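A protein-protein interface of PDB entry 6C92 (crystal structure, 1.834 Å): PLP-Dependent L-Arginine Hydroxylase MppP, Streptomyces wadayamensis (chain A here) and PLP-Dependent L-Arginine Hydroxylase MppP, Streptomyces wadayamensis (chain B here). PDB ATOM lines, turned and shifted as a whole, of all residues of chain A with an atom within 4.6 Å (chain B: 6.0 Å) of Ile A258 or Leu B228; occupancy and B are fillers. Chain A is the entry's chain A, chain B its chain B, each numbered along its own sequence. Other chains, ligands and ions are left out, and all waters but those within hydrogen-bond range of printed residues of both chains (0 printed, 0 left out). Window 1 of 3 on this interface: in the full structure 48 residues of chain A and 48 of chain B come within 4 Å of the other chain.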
ATOM      1  N   TRP A  49     -12.128 -17.304  11.444  1.00  0.00           N
ATOM      2  CA  TRP A  49     -13.047 -16.174  11.426  1.00  0.00           C
ATOM      3  C   TRP A  49     -13.525 -15.835  12.827  1.00  0.00           C
ATOM      4  O   TRP A  49     -13.518 -14.673  13.233  1.00  0.00           O
ATOM      5  CB  TRP A  49     -14.229 -16.485  10.515  1.00  0.00           C
ATOM      6  CG  TRP A  49     -15.086 -15.281  10.237  1.00  0.00           C
ATOM      7  CD1 TRP A  49     -15.902 -14.623  11.116  1.00  0.00           C
ATOM      8  CD2 TRP A  49     -15.215 -14.605   8.982  1.00  0.00           C
ATOM      9  NE1 TRP A  49     -16.503 -13.555  10.489  1.00  0.00           N
ATOM     10  CE2 TRP A  49     -16.114 -13.534   9.174  1.00  0.00           C
ATOM     11  CE3 TRP A  49     -14.639 -14.787   7.726  1.00  0.00           C
ATOM     12  CZ2 TRP A  49     -16.454 -12.646   8.147  1.00  0.00           C
ATOM     13  CZ3 TRP A  49     -14.981 -13.897   6.701  1.00  0.00           C
ATOM     14  CH2 TRP A  49     -15.874 -12.844   6.922  1.00  0.00           C
ATOM     15  N   LEU A 228      -4.279 -13.837  -0.662  1.00  0.00           N
ATOM     16  CA  LEU A 228      -4.470 -13.342   0.689  1.00  0.00           C
ATOM     17  C   LEU A 228      -3.100 -13.269   1.348  1.00  0.00           C
ATOM     18  O   LEU A 228      -2.420 -14.296   1.502  1.00  0.00           O
ATOM     19  CB  LEU A 228      -5.408 -14.260   1.457  1.00  0.00           C
ATOM     20  CG  LEU A 228      -6.816 -14.336   0.862  1.00  0.00           C
ATOM     21  CD1 LEU A 228      -7.583 -15.511   1.453  1.00  0.00           C
ATOM     22  CD2 LEU A 228      -7.582 -13.039   1.081  1.00  0.00           C
ATOM     23  N   LYS A 229      -2.668 -12.060   1.692  1.00  0.00           N
ATOM     24  CA  LYS A 229      -1.259 -11.837   1.965  1.00  0.00           C
ATOM     25  C   LYS A 229      -1.102 -10.501   2.676  1.00  0.00           C
ATOM     26  O   LYS A 229      -2.042  -9.712   2.785  1.00  0.00           O
ATOM     27  CB  LYS A 229      -0.450 -11.858   0.651  1.00  0.00           C
ATOM     28  CG  LYS A 229      -0.885 -10.690  -0.254  1.00  0.00           C
ATOM     29  CD  LYS A 229      -0.442 -10.811  -1.713  1.00  0.00           C
ATOM     30  CE  LYS A 229      -1.087  -9.690  -2.536  1.00  0.00           C
ATOM     31  NZ  LYS A 229      -0.771  -9.817  -3.996  1.00  0.00           N
ATOM     32  N   SER A 255      -6.808  -7.189   7.333  1.00  0.00           N
ATOM     33  CA  SER A 255      -7.830  -8.063   7.930  1.00  0.00           C
ATOM     34  C   SER A 255      -7.211  -8.967   8.986  1.00  0.00           C
ATOM     35  O   SER A 255      -6.188  -9.621   8.720  1.00  0.00           O
ATOM     36  CB  SER A 255      -8.490  -8.943   6.877  1.00  0.00           C
ATOM     37  OG  SER A 255      -9.303  -9.945   7.510  1.00  0.00           O
ATOM     38  N   PRO A 256      -7.805  -9.068  10.172  1.00  0.00           N
ATOM     39  CA  PRO A 256      -7.305 -10.049  11.136  1.00  0.00           C
ATOM     40  C   PRO A 256      -7.364 -11.484  10.627  1.00  0.00           C
ATOM     41  O   PRO A 256      -6.579 -12.323  11.079  1.00  0.00           O
ATOM     42  CB  PRO A 256      -8.229  -9.863  12.350  1.00  0.00           C
ATOM     43  CG  PRO A 256      -9.463  -9.208  11.805  1.00  0.00           C
ATOM     44  CD  PRO A 256      -8.967  -8.316  10.682  1.00  0.00           C
ATOM     45  N   LEU A 257      -8.295 -11.800   9.734  1.00  0.00           N
ATOM     46  CA  LEU A 257      -8.353 -13.147   9.178  1.00  0.00           C
ATOM     47  C   LEU A 257      -7.125 -13.430   8.332  1.00  0.00           C
ATOM     48  O   LEU A 257      -6.584 -14.539   8.352  1.00  0.00           O
ATOM     49  CB  LEU A 257      -9.623 -13.312   8.351  1.00  0.00           C
ATOM     50  CG  LEU A 257      -9.859 -14.721   7.799  1.00  0.00           C
ATOM     51  CD1 LEU A 257     -10.215 -15.662   8.928  1.00  0.00           C
ATOM     52  CD2 LEU A 257     -10.943 -14.771   6.784  1.00  0.00           C
ATOM     53  N   ILE A 258      -6.670 -12.449   7.560  1.00  0.00           N
ATOM     54  CA  ILE A 258      -5.461 -12.660   6.776  1.00  0.00           C
ATOM     55  C   ILE A 258      -4.259 -12.810   7.703  1.00  0.00           C
ATOM     56  O   ILE A 258      -3.366 -13.630   7.461  1.00  0.00           O
ATOM     57  CB  ILE A 258      -5.268 -11.519   5.758  1.00  0.00           C
ATOM     58  CG1 ILE A 258      -6.373 -11.582   4.692  1.00  0.00           C
ATOM     59  CG2 ILE A 258      -3.840 -11.559   5.175  1.00  0.00           C
ATOM     60  CD1 ILE A 258      -6.415 -10.394   3.684  1.00  0.00           C
ATOM     61  N   LEU A 259      -4.202 -12.012   8.766  1.00  0.00           N
ATOM     62  CA  LEU A 259      -3.096 -12.152   9.715  1.00  0.00           C
ATOM     63  C   LEU A 259      -3.124 -13.535  10.362  1.00  0.00           C
ATOM     64  O   LEU A 259      -2.086 -14.195  10.508  1.00  0.00           O
ATOM     65  CB  LEU A 259      -3.205 -11.077  10.786  1.00  0.00           C
ATOM     66  CG  LEU A 259      -2.416  -9.757  10.800  1.00  0.00           C
ATOM     67  CD1 LEU A 259      -1.461  -9.505   9.671  1.00  0.00           C
ATOM     68  CD2 LEU A 259      -3.318  -8.620  11.026  1.00  0.00           C
ATOM     69  N   ALA A 260      -4.306 -13.990  10.760  1.00  0.00           N
ATOM     70  CA  ALA A 260      -4.410 -15.328  11.344  1.00  0.00           C
ATOM     71  C   ALA A 260      -3.984 -16.386  10.341  1.00  0.00           C
ATOM     72  O   ALA A 260      -3.287 -17.340  10.691  1.00  0.00           O
ATOM     73  CB  ALA A 260      -5.834 -15.581  11.834  1.00  0.00           C
ATOM     74  N   LEU A 261      -4.373 -16.224   9.077  1.00  0.00           N
ATOM     75  CA  LEU A 261      -3.938 -17.147   8.030  1.00  0.00           C
ATOM     76  C   LEU A 261      -2.423 -17.177   7.870  1.00  0.00           C
ATOM     77  O   LEU A 261      -1.822 -18.254   7.728  1.00  0.00           O
ATOM     78  CB  LEU A 261      -4.602 -16.735   6.720  1.00  0.00           C
ATOM     79  CG  LEU A 261      -4.916 -17.749   5.637  1.00  0.00           C
ATOM     80  CD1 LEU A 261      -5.838 -18.819   6.159  1.00  0.00           C
ATOM     81  CD2 LEU A 261      -5.585 -17.034   4.484  1.00  0.00           C
ATOM     82  N   ILE A 262      -1.786 -16.003   7.866  1.00  0.00           N
ATOM     83  CA  ILE A 262      -0.327 -15.933   7.805  1.00  0.00           C
ATOM     84  C   ILE A 262       0.289 -16.660   8.984  1.00  0.00           C
ATOM     85  O   ILE A 262       1.274 -17.395   8.830  1.00  0.00           O
ATOM     86  CB  ILE A 262       0.125 -14.465   7.749  1.00  0.00           C
ATOM     87  CG1 ILE A 262      -0.257 -13.906   6.384  1.00  0.00           C
ATOM     88  CG2 ILE A 262       1.647 -14.298   8.069  1.00  0.00           C
ATOM     89  CD1 ILE A 262      -0.171 -12.422   6.285  1.00  0.00           C
ATOM     90  N   THR B 219     -16.992  -1.834  -0.828  1.00  0.00           N
ATOM     91  CA  THR B 219     -17.843  -2.824  -0.197  1.00  0.00           C
ATOM     92  C   THR B 219     -17.583  -2.893   1.288  1.00  0.00           C
ATOM     93  O   THR B 219     -18.348  -3.543   2.002  1.00  0.00           O
ATOM     94  CB  THR B 219     -17.630  -4.219  -0.801  1.00  0.00           C
ATOM     95  OG1 THR B 219     -16.351  -4.740  -0.402  1.00  0.00           O
ATOM     96  CG2 THR B 219     -17.702  -4.193  -2.278  1.00  0.00           C
ATOM     97  N   GLY B 220     -16.546  -2.207   1.759  1.00  0.00           N
ATOM     98  CA  GLY B 220     -15.999  -2.447   3.086  1.00  0.00           C
ATOM     99  C   GLY B 220     -16.801  -1.976   4.276  1.00  0.00           C
ATOM    100  O   GLY B 220     -16.554  -2.455   5.373  1.00  0.00           O
ATOM    101  N   THR B 225     -17.222  -8.069   7.571  1.00  0.00           N
ATOM    102  CA  THR B 225     -16.404  -9.055   6.881  1.00  0.00           C
ATOM    103  C   THR B 225     -14.940  -9.008   7.313  1.00  0.00           C
ATOM    104  O   THR B 225     -14.064  -9.428   6.544  1.00  0.00           O
ATOM    105  CB  THR B 225     -16.486  -8.848   5.378  1.00  0.00           C
ATOM    106  OG1 THR B 225     -16.036  -7.528   5.089  1.00  0.00           O
ATOM    107  CG2 THR B 225     -17.899  -9.018   4.851  1.00  0.00           C
ATOM    108  N   LEU B 226     -14.646  -8.506   8.514  1.00  0.00           N
ATOM    109  CA  LEU B 226     -13.274  -8.523   9.017  1.00  0.00           C
ATOM    110  C   LEU B 226     -12.344  -7.794   8.055  1.00  0.00           C
ATOM    111  O   LEU B 226     -11.199  -8.201   7.823  1.00  0.00           O
ATOM    112  CB  LEU B 226     -12.783  -9.947   9.235  1.00  0.00           C
ATOM    113  CG  LEU B 226     -13.648 -10.761  10.204  1.00  0.00           C
ATOM    114  CD1 LEU B 226     -13.126 -12.163  10.259  1.00  0.00           C
ATOM    115  CD2 LEU B 226     -13.623 -10.108  11.582  1.00  0.00           C
ATOM    116  N   ASP B 227     -12.847  -6.714   7.484  1.00  0.00           N
ATOM    117  CA  ASP B 227     -12.085  -5.881   6.560  1.00  0.00           C
ATOM    118  C   ASP B 227     -11.712  -6.585   5.261  1.00  0.00           C
ATOM    119  O   ASP B 227     -10.807  -6.129   4.544  1.00  0.00           O
ATOM    120  CB  ASP B 227     -10.830  -5.336   7.242  1.00  0.00           C
ATOM    121  CG  ASP B 227     -11.094  -4.002   7.872  1.00  0.00           C
ATOM    122  OD1 ASP B 227     -11.140  -3.009   7.114  1.00  0.00           O
ATOM    123  OD2 ASP B 227     -11.343  -3.968   9.091  1.00  0.00           O
ATOM    124  N   LEU B 228     -12.405  -7.662   4.918  1.00  0.00           N
ATOM    125  CA  LEU B 228     -12.272  -8.300   3.622  1.00  0.00           C
ATOM    126  C   LEU B 228     -13.222  -7.577   2.672  1.00  0.00           C
ATOM    127  O   LEU B 228     -14.429  -7.593   2.873  1.00  0.00           O
ATOM    128  CB  LEU B 228     -12.591  -9.788   3.725  1.00  0.00           C
ATOM    129  CG  LEU B 228     -11.639 -10.569   4.638  1.00  0.00           C
ATOM    130  CD1 LEU B 228     -12.239 -11.922   4.888  1.00  0.00           C
ATOM    131  CD2 LEU B 228     -10.224 -10.697   4.041  1.00  0.00           C
ATOM    132  N   LYS B 229     -12.671  -6.902   1.671  1.00  0.00           N
ATOM    133  CA  LYS B 229     -13.416  -5.880   0.955  1.00  0.00           C
ATOM    134  C   LYS B 229     -12.692  -5.600  -0.352  1.00  0.00           C
ATOM    135  O   LYS B 229     -11.574  -6.069  -0.577  1.00  0.00           O
ATOM    136  CB  LYS B 229     -13.521  -4.612   1.798  1.00  0.00           C
ATOM    137  CG  LYS B 229     -12.111  -3.968   2.009  1.00  0.00           C
ATOM    138  CD  LYS B 229     -12.048  -3.064   3.207  1.00  0.00           C
ATOM    139  CE  LYS B 229     -10.595  -2.714   3.529  1.00  0.00           C
ATOM    140  NZ  LYS B 229     -10.474  -1.707   4.623  1.00  0.00           N
ATOM    141  N   ALA B 230     -13.324  -4.787  -1.191  1.00  0.00           N
ATOM    142  CA  ALA B 230     -12.651  -4.209  -2.340  1.00  0.00           C
ATOM    143  C   ALA B 230     -13.135  -2.777  -2.526  1.00  0.00           C
ATOM    144  O   ALA B 230     -14.297  -2.450  -2.272  1.00  0.00           O
ATOM    145  CB  ALA B 230     -12.908  -5.007  -3.629  1.00  0.00           C
ATOM    146  N   ILE B 258     -12.119 -13.002  -1.914  1.00  0.00           N
ATOM    147  CA  ILE B 258     -12.795 -11.792  -1.485  1.00  0.00           C
ATOM    148  C   ILE B 258     -13.905 -11.437  -2.459  1.00  0.00           C
ATOM    149  O   ILE B 258     -14.997 -11.014  -2.053  1.00  0.00           O
ATOM    150  CB  ILE B 258     -11.759 -10.657  -1.329  1.00  0.00           C
ATOM    151  CG1 ILE B 258     -10.871 -10.954  -0.124  1.00  0.00           C
ATOM    152  CG2 ILE B 258     -12.445  -9.293  -1.208  1.00  0.00           C
ATOM    153  CD1 ILE B 258      -9.668 -10.020   0.027  1.00  0.00           C
ATOM    154  N   LEU B 261     -16.711 -13.647  -1.771  1.00  0.00           N
ATOM    155  CA  LEU B 261     -17.385 -13.203  -0.553  1.00  0.00           C
ATOM    156  C   LEU B 261     -18.291 -12.018  -0.838  1.00  0.00           C
ATOM    157  O   LEU B 261     -19.407 -11.927  -0.304  1.00  0.00           O
ATOM    158  CB  LEU B 261     -16.358 -12.783   0.508  1.00  0.00           C
ATOM    159  CG  LEU B 261     -15.971 -13.514   1.783  1.00  0.00           C
ATOM    160  CD1 LEU B 261     -17.002 -14.546   2.227  1.00  0.00           C
ATOM    161  CD2 LEU B 261     -14.610 -14.117   1.613  1.00  0.00           C
ATOM    162  N   ILE B 262     -17.799 -11.066  -1.639  1.00  0.00           N
ATOM    163  CA  ILE B 262     -18.603  -9.899  -1.984  1.00  0.00           C
ATOM    164  C   ILE B 262     -19.848 -10.333  -2.741  1.00  0.00           C
ATOM    165  O   ILE B 262     -20.953  -9.833  -2.501  1.00  0.00           O
ATOM    166  CB  ILE B 262     -17.769  -8.899  -2.807  1.00  0.00           C
ATOM    167  CG1 ILE B 262     -16.747  -8.221  -1.907  1.00  0.00           C
ATOM    168  CG2 ILE B 262     -18.674  -7.868  -3.495  1.00  0.00           C
ATOM    169  CD1 ILE B 262     -15.727  -7.421  -2.691  1.00  0.00           C
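The side-chain hydroxyl (OG) of Ser A255 sits at hydrogen-bond distance from the backbone carbonyl oxygen (O) of Leu B226, 2.6 Å away.
The side-chain hydroxyl (OG1) of Thr B225 sits at hydrogen-bond distance from the backbone carbonyl oxygen (O) of Leu B228 (2.7 Å). The side-chain hydroxyl (OG) of Ser A255 is in hydrogen-bond range of the backbone NH (N) of Leu A257.
Among the printed residues, merely in contact across the chains: Trp A49 with Leu B226 (3.5 Å), Pro A256 with Leu B226 (3.6 Å), Leu A257 with Leu B228 (3.7 Å), Ser A255 with Leu B228 (3.7 Å), Trp A49 with Thr B225 (3.8 Å), Leu A228 with Ile B258 (3.8 Å), Trp A49 with Leu B228 (3.8 Å) and Ile A258 with Leu B228 (3.8 Å).
Ile A258 touches just one residue of chain B: Leu B228. Of chain A, only Trp A49 (3.8 Å), Ser A255 (3.7 Å), Leu A257 (3.7 Å) and Ile A258 (3.8 Å) come within 4 Å of Leu B228. Printed residues of chain B within 4 Å of Ser A255: Leu B226 and Leu B228. Of the printed residues of chain B, Leu A228 touches Ile B258 (3.8 Å). Of the printed residues of chain A, Thr B225 touches Trp A49 (3.8 Å). Ile A262 touches none of the printed residues of chain B. Asp B227 touches none of the printed residues of chain A. The nearest printed residue of chain A that does not touch Leu B228 is Leu A228 (4.6 Å).
Of the 11 printed residues of chain B, 4 touch a printed residue of chain A. Printed residues of chain B that touch a printed residue of chain A: Thr B225, Leu B226, Leu B228 and Ile B258. Hydrophobic or aromatic side chains of chain B within 4 Å of the printed part of chain A: Leu B226, Leu B228 and Ile B258.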
